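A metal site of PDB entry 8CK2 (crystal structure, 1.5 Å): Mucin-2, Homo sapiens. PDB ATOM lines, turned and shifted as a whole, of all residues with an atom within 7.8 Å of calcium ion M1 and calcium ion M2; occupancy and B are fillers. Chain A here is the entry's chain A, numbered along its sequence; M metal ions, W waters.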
ATOM      1  N   ILE A  10      37.350  18.598 -15.205  1.00  0.00           N
ATOM      2  CA  ILE A  10      36.164  18.301 -15.992  1.00  0.00           C
ATOM      3  C   ILE A  10      35.116  19.358 -15.666  1.00  0.00           C
ATOM      4  O   ILE A  10      34.780  19.561 -14.500  1.00  0.00           O
ATOM      5  CB  ILE A  10      35.639  16.891 -15.671  1.00  0.00           C
ATOM      6  CG1 ILE A  10      36.687  15.834 -15.997  1.00  0.00           C
ATOM      7  CG2 ILE A  10      34.353  16.594 -16.456  1.00  0.00           C
ATOM      8  CD1 ILE A  10      36.532  14.591 -15.165  1.00  0.00           C
ATOM      9  N   ASN A  11      34.590  20.016 -16.703  1.00  0.00           N
ATOM     10  CA  ASN A  11      33.589  21.057 -16.486  1.00  0.00           C
ATOM     11  C   ASN A  11      32.711  21.101 -17.739  1.00  0.00           C
ATOM     12  O   ASN A  11      32.869  21.968 -18.594  1.00  0.00           O
ATOM     13  CB  ASN A  11      34.208  22.436 -16.204  1.00  0.00           C
ATOM     14  CG  ASN A  11      33.161  23.454 -15.819  1.00  0.00           C
ATOM     15  OD1 ASN A  11      32.019  23.087 -15.523  1.00  0.00           O
ATOM     16  ND2 ASN A  11      33.534  24.740 -15.829  1.00  0.00           N
ATOM     17  N   GLU A  12      31.784  20.141 -17.828  1.00  0.00           N
ATOM     18  CA  GLU A  12      30.979  19.970 -19.028  1.00  0.00           C
ATOM     19  C   GLU A  12      29.569  20.511 -18.894  1.00  0.00           C
ATOM     20  O   GLU A  12      28.906  20.749 -19.905  1.00  0.00           O
ATOM     21  CB  GLU A  12      30.889  18.486 -19.395  1.00  0.00           C
ATOM     22  CG  GLU A  12      32.255  17.922 -19.739  1.00  0.00           C
ATOM     23  CD  GLU A  12      32.653  18.219 -21.168  1.00  0.00           C
ATOM     24  OE1 GLU A  12      32.046  17.636 -22.081  1.00  0.00           O
ATOM     25  OE2 GLU A  12      33.574  19.052 -21.372  1.00  0.00           O
ATOM     26  N   ASP A  13      29.094  20.697 -17.666  1.00  0.00           N
ATOM     27  CA  ASP A  13      27.777  21.259 -17.391  1.00  0.00           C
ATOM     28  C   ASP A  13      27.993  22.625 -16.773  1.00  0.00           C
ATOM     29  O   ASP A  13      29.111  22.945 -16.339  1.00  0.00           O
ATOM     30  CB  ASP A  13      27.012  20.332 -16.428  1.00  0.00           C
ATOM     31  CG  ASP A  13      25.523  20.653 -16.318  1.00  0.00           C
ATOM     32  OD1 ASP A  13      24.942  21.488 -17.049  1.00  0.00           O
ATOM     33  OD2 ASP A  13      24.915  20.029 -15.437  1.00  0.00           O
ATOM     34  N   HIS A  14      26.930  23.425 -16.724  1.00  0.00           N
ATOM     35  CA  HIS A  14      26.997  24.728 -16.088  1.00  0.00           C
ATOM     36  C   HIS A  14      25.616  25.050 -15.537  1.00  0.00           C
ATOM     37  O   HIS A  14      24.617  24.554 -16.069  1.00  0.00           O
ATOM     38  CB  HIS A  14      27.450  25.823 -17.075  1.00  0.00           C
ATOM     39  CG  HIS A  14      28.675  25.454 -17.853  1.00  0.00           C
ATOM     40  ND1 HIS A  14      29.946  25.554 -17.328  1.00  0.00           N
ATOM     41  CD2 HIS A  14      28.812  24.922 -19.093  1.00  0.00           C
ATOM     42  CE1 HIS A  14      30.819  25.136 -18.232  1.00  0.00           C
ATOM     43  NE2 HIS A  14      30.158  24.751 -19.306  1.00  0.00           N
ATOM     44  N   PRO A  15      25.535  25.883 -14.490  1.00  0.00           N
ATOM     45  CA  PRO A  15      24.238  26.083 -13.800  1.00  0.00           C
ATOM     46  C   PRO A  15      23.136  26.648 -14.657  1.00  0.00           C
ATOM     47  O   PRO A  15      21.974  26.452 -14.323  1.00  0.00           O
ATOM     48  CB  PRO A  15      24.587  27.081 -12.684  1.00  0.00           C
ATOM     49  CG  PRO A  15      26.044  26.876 -12.429  1.00  0.00           C
ATOM     50  CD  PRO A  15      26.647  26.536 -13.776  1.00  0.00           C
ATOM     51  N   SER A  16      23.460  27.400 -15.714  1.00  0.00           N
ATOM     52  CA  SER A  16      22.438  27.939 -16.586  1.00  0.00           C
ATOM     53  C   SER A  16      22.521  27.367 -17.998  1.00  0.00           C
ATOM     54  O   SER A  16      22.087  28.027 -18.947  1.00  0.00           O
ATOM     55  CB  SER A  16      22.499  29.464 -16.630  1.00  0.00           C
ATOM     56  OG  SER A  16      22.464  30.034 -15.331  1.00  0.00           O
ATOM     57  N   SER A  17      23.084  26.176 -18.153  1.00  0.00           N
ATOM     58  CA  SER A  17      23.180  25.486 -19.433  1.00  0.00           C
ATOM     59  C   SER A  17      22.499  24.125 -19.329  1.00  0.00           C
ATOM     60  O   SER A  17      22.425  23.527 -18.250  1.00  0.00           O
ATOM     61  CB  SER A  17      24.642  25.301 -19.876  1.00  0.00           C
ATOM     62  OG  SER A  17      25.410  26.469 -19.663  1.00  0.00           O
ATOM     63  N   GLY A  18      22.017  23.623 -20.462  1.00  0.00           N
ATOM     64  CA  GLY A  18      21.354  22.335 -20.446  1.00  0.00           C
ATOM     65  C   GLY A  18      19.967  22.417 -19.832  1.00  0.00           C
ATOM     66  O   GLY A  18      19.385  23.488 -19.633  1.00  0.00           O
ATOM     67  N   SER A  19      19.440  21.227 -19.508  1.00  0.00           N
ATOM     68  CA  SER A  19      18.059  21.068 -19.086  1.00  0.00           C
ATOM     69  C   SER A  19      17.913  20.585 -17.640  1.00  0.00           C
ATOM     70  O   SER A  19      16.783  20.319 -17.207  1.00  0.00           O
ATOM     71  CB  SER A  19      17.344  20.090 -20.028  1.00  0.00           C
ATOM     72  OG  SER A  19      17.922  18.802 -19.954  1.00  0.00           O
ATOM     73  N   ASP A  20      19.010  20.487 -16.883  1.00  0.00           N
ATOM     74  CA  ASP A  20      18.961  19.840 -15.583  1.00  0.00           C
ATOM     75  C   ASP A  20      18.771  20.809 -14.424  1.00  0.00           C
ATOM     76  O   ASP A  20      18.658  20.346 -13.279  1.00  0.00           O
ATOM     77  CB  ASP A  20      20.220  18.971 -15.371  1.00  0.00           C
ATOM     78  CG  ASP A  20      21.535  19.768 -15.457  1.00  0.00           C
ATOM     79  OD1 ASP A  20      21.567  20.902 -15.984  1.00  0.00           O
ATOM     80  OD2 ASP A  20      22.558  19.221 -14.988  1.00  0.00           O
ATOM     81  N   ASP A  21      18.708  22.113 -14.702  1.00  0.00           N
ATOM     82  CA  ASP A  21      18.555  23.133 -13.652  1.00  0.00           C
ATOM     83  C   ASP A  21      19.531  22.918 -12.505  1.00  0.00           C
ATOM     84  O   ASP A  21      19.157  22.808 -11.331  1.00  0.00           O
ATOM     85  CB  ASP A  21      17.115  23.181 -13.153  1.00  0.00           C
ATOM     86  CG  ASP A  21      16.858  24.393 -12.275  1.00  0.00           C
ATOM     87  OD1 ASP A  21      17.324  25.488 -12.632  1.00  0.00           O
ATOM     88  OD2 ASP A  21      16.181  24.216 -11.237  1.00  0.00           O
ATOM     89  N   GLY A  22      20.804  22.810 -12.874  1.00  0.00           N
ATOM     90  CA  GLY A  22      21.856  22.637 -11.886  1.00  0.00           C
ATOM     91  C   GLY A  22      23.173  22.396 -12.585  1.00  0.00           C
ATOM     92  O   GLY A  22      23.346  22.706 -13.759  1.00  0.00           O
ATOM     93  N   ASP A  23      24.112  21.818 -11.840  1.00  0.00           N
ATOM     94  CA  ASP A  23      25.453  21.533 -12.350  1.00  0.00           C
ATOM     95  C   ASP A  23      25.809  20.121 -11.941  1.00  0.00           C
ATOM     96  O   ASP A  23      25.907  19.822 -10.746  1.00  0.00           O
ATOM     97  CB  ASP A  23      26.490  22.526 -11.817  1.00  0.00           C
ATOM     98  CG  ASP A  23      27.793  22.493 -12.605  1.00  0.00           C
ATOM     99  OD1 ASP A  23      27.737  22.349 -13.844  1.00  0.00           O
ATOM    100  OD2 ASP A  23      28.866  22.589 -11.999  1.00  0.00           O
ATOM    101  N   ARG A  24      25.963  19.237 -12.927  1.00  0.00           N
ATOM    102  CA  ARG A  24      26.355  17.867 -12.699  1.00  0.00           C
ATOM    103  C   ARG A  24      27.620  17.588 -13.480  1.00  0.00           C
ATOM    104  O   ARG A  24      27.733  17.943 -14.654  1.00  0.00           O
ATOM    105  CB  ARG A  24      25.231  16.894 -13.109  1.00  0.00           C
ATOM    106  CG  ARG A  24      25.656  15.439 -13.242  1.00  0.00           C
ATOM    107  CD  ARG A  24      24.645  14.500 -12.578  1.00  0.00           C
ATOM    108  NE  ARG A  24      25.031  13.105 -12.626  1.00  0.00           N
ATOM    109  CZ  ARG A  24      26.126  12.592 -12.065  1.00  0.00           C
ATOM    110  NH1 ARG A  24      26.996  13.363 -11.412  1.00  0.00           N
ATOM    111  NH2 ARG A  24      26.361  11.285 -12.157  1.00  0.00           N
ATOM    112  N   GLU A  25      28.598  16.973 -12.820  1.00  0.00           N
ATOM    113  CA  GLU A  25      29.836  16.563 -13.486  1.00  0.00           C
ATOM    114  C   GLU A  25      30.089  15.089 -13.249  1.00  0.00           C
ATOM    115  O   GLU A  25      29.995  14.608 -12.113  1.00  0.00           O
ATOM    116  CB  GLU A  25      31.052  17.380 -13.030  1.00  0.00           C
ATOM    117  CG  GLU A  25      30.920  18.924 -13.205  1.00  0.00           C
ATOM    118  CD  GLU A  25      30.806  19.369 -14.662  1.00  0.00           C
ATOM    119  OE1 GLU A  25      31.181  18.577 -15.565  1.00  0.00           O
ATOM    120  OE2 GLU A  25      30.365  20.515 -14.906  1.00  0.00           O
ATOM    121  N   ARG A  40      35.211  21.444  -6.972  1.00  0.00           N
ATOM    122  CA  ARG A  40      35.572  22.805  -6.626  1.00  0.00           C
ATOM    123  C   ARG A  40      34.749  23.802  -7.440  1.00  0.00           C
ATOM    124  O   ARG A  40      34.445  23.555  -8.601  1.00  0.00           O
ATOM    125  CB  ARG A  40      37.055  23.080  -6.896  1.00  0.00           C
ATOM    126  CG  ARG A  40      38.018  22.273  -6.040  1.00  0.00           C
ATOM    127  CD  ARG A  40      37.917  22.654  -4.574  1.00  0.00           C
ATOM    128  NE  ARG A  40      38.660  21.720  -3.728  1.00  0.00           N
ATOM    129  CZ  ARG A  40      39.927  21.878  -3.374  1.00  0.00           C
ATOM    130  NH1 ARG A  40      40.634  22.924  -3.770  1.00  0.00           N
ATOM    131  NH2 ARG A  40      40.519  20.945  -2.623  1.00  0.00           N
ATOM    132  N   VAL A  42      34.292  27.018  -9.749  1.00  0.00           N
ATOM    133  CA  VAL A  42      35.158  27.622 -10.756  1.00  0.00           C
ATOM    134  C   VAL A  42      35.681  28.965 -10.279  1.00  0.00           C
ATOM    135  O   VAL A  42      36.845  29.310 -10.508  1.00  0.00           O
ATOM    136  CB  VAL A  42      34.419  27.727 -12.094  1.00  0.00           C
ATOM    137  CG1 VAL A  42      35.183  28.622 -13.061  1.00  0.00           C
ATOM    138  CG2 VAL A  42      34.193  26.339 -12.689  1.00  0.00           C
ATOM    139  N   PHE A  64      29.648  14.527  -9.222  1.00  0.00           N
ATOM    140  CA  PHE A  64      29.214  15.778  -8.610  1.00  0.00           C
ATOM    141  C   PHE A  64      27.793  16.105  -9.030  1.00  0.00           C
ATOM    142  O   PHE A  64      27.478  16.072 -10.222  1.00  0.00           O
ATOM    143  CB  PHE A  64      30.130  16.937  -9.013  1.00  0.00           C
ATOM    144  CG  PHE A  64      29.696  18.236  -8.411  1.00  0.00           C
ATOM    145  CD1 PHE A  64      30.032  18.527  -7.110  1.00  0.00           C
ATOM    146  CD2 PHE A  64      28.925  19.137  -9.140  1.00  0.00           C
ATOM    147  CE1 PHE A  64      29.608  19.695  -6.536  1.00  0.00           C
ATOM    148  CE2 PHE A  64      28.492  20.311  -8.553  1.00  0.00           C
ATOM    149  CZ  PHE A  64      28.828  20.588  -7.246  1.00  0.00           C
ATOM    150  N   CYS A  66      24.884  19.256  -8.179  1.00  0.00           N
ATOM    151  CA  CYS A  66      24.272  20.408  -7.521  1.00  0.00           C
ATOM    152  C   CYS A  66      22.946  20.703  -8.202  1.00  0.00           C
ATOM    153  O   CYS A  66      22.889  20.765  -9.432  1.00  0.00           O
ATOM    154  CB  CYS A  66      25.204  21.619  -7.613  1.00  0.00           C
ATOM    155  SG  CYS A  66      24.615  23.116  -6.748  1.00  0.00           S
ATOM    156  N   ASN A  68      19.833  23.464  -8.560  1.00  0.00           N
ATOM    157  CA  ASN A  68      19.681  24.905  -8.307  1.00  0.00           C
ATOM    158  C   ASN A  68      18.663  25.197  -7.204  1.00  0.00           C
ATOM    159  O   ASN A  68      18.855  26.128  -6.415  1.00  0.00           O
ATOM    160  CB  ASN A  68      19.279  25.625  -9.594  1.00  0.00           C
ATOM    161  CG  ASN A  68      20.438  25.785 -10.553  1.00  0.00           C
ATOM    162  OD1 ASN A  68      21.597  25.743 -10.147  1.00  0.00           O
ATOM    163  ND2 ASN A  68      20.130  25.965 -11.821  1.00  0.00           N
ATOM    164  N   TYR A  81      26.587  27.597  -7.897  1.00  0.00           N
ATOM    165  CA  TYR A  81      27.832  27.997  -8.546  1.00  0.00           C
ATOM    166  C   TYR A  81      28.132  27.029  -9.685  1.00  0.00           C
ATOM    167  O   TYR A  81      27.617  25.907  -9.738  1.00  0.00           O
ATOM    168  CB  TYR A  81      29.013  27.945  -7.559  1.00  0.00           C
ATOM    169  CG  TYR A  81      28.885  28.835  -6.350  1.00  0.00           C
ATOM    170  CD1 TYR A  81      28.316  30.086  -6.442  1.00  0.00           C
ATOM    171  CD2 TYR A  81      29.334  28.391  -5.110  1.00  0.00           C
ATOM    172  CE1 TYR A  81      28.216  30.912  -5.308  1.00  0.00           C
ATOM    173  CE2 TYR A  81      29.234  29.194  -3.976  1.00  0.00           C
ATOM    174  CZ  TYR A  81      28.675  30.445  -4.091  1.00  0.00           C
ATOM    175  OH  TYR A  81      28.565  31.243  -2.970  1.00  0.00           O
ATOM    176  N   ASP A  82      29.021  27.430 -10.590  1.00  0.00           N
ATOM    177  CA  ASP A  82      29.555  26.468 -11.555  1.00  0.00           C
ATOM    178  C   ASP A  82      30.684  25.706 -10.891  1.00  0.00           C
ATOM    179  O   ASP A  82      31.584  26.320 -10.279  1.00  0.00           O
ATOM    180  CB  ASP A  82      30.065  27.163 -12.821  1.00  0.00           C
ATOM    181  CG  ASP A  82      30.336  26.182 -13.954  1.00  0.00           C
ATOM    182  OD1 ASP A  82      29.863  25.027 -13.869  1.00  0.00           O
ATOM    183  OD2 ASP A  82      31.023  26.558 -14.922  1.00  0.00           O
ATOM    184  N   TYR A  83      30.658  24.374 -11.021  1.00  0.00           N
ATOM    185  CA  TYR A  83      31.666  23.531 -10.393  1.00  0.00           C
ATOM    186  C   TYR A  83      32.407  22.742 -11.470  1.00  0.00           C
ATOM    187  O   TYR A  83      31.924  22.566 -12.592  1.00  0.00           O
ATOM    188  CB  TYR A  83      31.053  22.543  -9.396  1.00  0.00           C
ATOM    189  CG  TYR A  83      30.465  23.216  -8.168  1.00  0.00           C
ATOM    190  CD1 TYR A  83      29.182  23.745  -8.197  1.00  0.00           C
ATOM    191  CD2 TYR A  83      31.181  23.269  -6.976  1.00  0.00           C
ATOM    192  CE1 TYR A  83      28.632  24.352  -7.090  1.00  0.00           C
ATOM    193  CE2 TYR A  83      30.622  23.877  -5.846  1.00  0.00           C
ATOM    194  CZ  TYR A  83      29.367  24.409  -5.930  1.00  0.00           C
ATOM    195  OH  TYR A  83      28.818  24.986  -4.803  1.00  0.00           O
ATOM    196  N   LYS A  84      33.598  22.296 -11.078  1.00  0.00           N
ATOM    197  CA  LYS A  84      34.485  21.487 -11.902  1.00  0.00           C
ATOM    198  C   LYS A  84      35.070  20.383 -11.022  1.00  0.00           C
ATOM    199  O   LYS A  84      35.155  20.536  -9.801  1.00  0.00           O
ATOM    200  CB  LYS A  84      35.598  22.343 -12.509  1.00  0.00           C
ATOM    201  CG  LYS A  84      36.407  23.132 -11.425  1.00  0.00           C
ATOM    202  CD  LYS A  84      37.520  23.979 -12.058  1.00  0.00           C
ATOM    203  CE  LYS A  84      38.550  24.446 -11.021  1.00  0.00           C
ATOM    204  NZ  LYS A  84      39.623  25.339 -11.588  1.00  0.00           N
ATOM    205  N   ILE A  85      35.443  19.253 -11.631  1.00  0.00           N
ATOM    206  CA  ILE A  85      35.966  18.164 -10.830  1.00  0.00           C
ATOM    207  C   ILE A  85      37.256  17.617 -11.440  1.00  0.00           C
ATOM    208  O   ILE A  85      37.490  17.698 -12.646  1.00  0.00           O
ATOM    209  CB  ILE A  85      34.965  17.004 -10.657  1.00  0.00           C
ATOM    210  CG1 ILE A  85      34.690  16.301 -12.000  1.00  0.00           C
ATOM    211  CG2 ILE A  85      33.666  17.511 -10.032  1.00  0.00           C
ATOM    212  CD1 ILE A  85      33.929  14.957 -11.887  1.00  0.00           C
HETATM  213 CA    CA M   1      30.159  22.659 -14.198  1.00  0.00          CA
HETATM  214 CA    CA M   2      23.065  22.813 -16.135  1.00  0.00          CA
HETATM  215  O   HOH W   1      21.161  24.118 -15.484  1.00  0.00           O
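The backbone NH (N) of His 14 lies close to the side-chain carboxylate (OD1) of Asp 23, 3.2 Å away.
The backbone NH (N) of Gly 22 lies close to the side-chain amide nitrogen (ND2) of Asn 68.
OD2 of Asp 13 lies within hydrogen-bond range of N of Arg 24.
O of Asp 82 lies within hydrogen-bond range of N of Val 42 (2.8 Å).
O of Asp 23 sits at hydrogen-bond distance from N of Cys 66 (2.8 Å).
OE1 of Glu 25 sits at hydrogen-bond distance from N of Glu 12 (2.8 Å).
O of Glu 25 lies within hydrogen-bond range of N of Phe 64 (2.9 Å).
A ring nitrogen (ND1) of His 14 lies within hydrogen-bond range of the side-chain carboxylate (OD2) of Asp 82 (2.8 Å).
Along chain A the residues within 4 Å of calcium ion M1 span positions 11 to 83.
Of the 26 residues printed, 5 come within 4 Å of calcium ion M2.
The nearest printed residue that does not touch calcium ion M2 is Pro 15 (4.1 Å).
Calcium ion M1 is bound by the side-chain carboxylate (OE2) of Glu 25, the side-chain amide oxygen (OD1) of Asn 11, the backbone carbonyl oxygen (O) of Tyr 83, the backbone carbonyl oxygen (O) of Asp 13, the side-chain carboxylate (OD1) of Asp 82, the side-chain carboxylate (OD1) of Asp 23 and the side-chain carboxylate (OD2) of Asp 23.
O of Ser 17 binds calcium ion M2, 2.3 Å away.
Calcium ion M2 is bound by O of His 14 (2.3 Å).
O of Gly 22 binds calcium ion M2 (2.4 Å).
Calcium ion M2 is bound by water W1, at 2.4 Å.
OD1 of Asp 20 is bound to calcium ion M2 (2.4 Å).
Calcium ion M2 is bound by the side-chain carboxylate (OD1) of Asp 13, 2.5 Å away.
Water W1 lies within hydrogen-bond range of the backbone carbonyl oxygen of Pro 15 (2.7 Å), the backbone NH of Gly 22 (2.9 Å) and the backbone NH of Asp 21 (3.3 Å).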
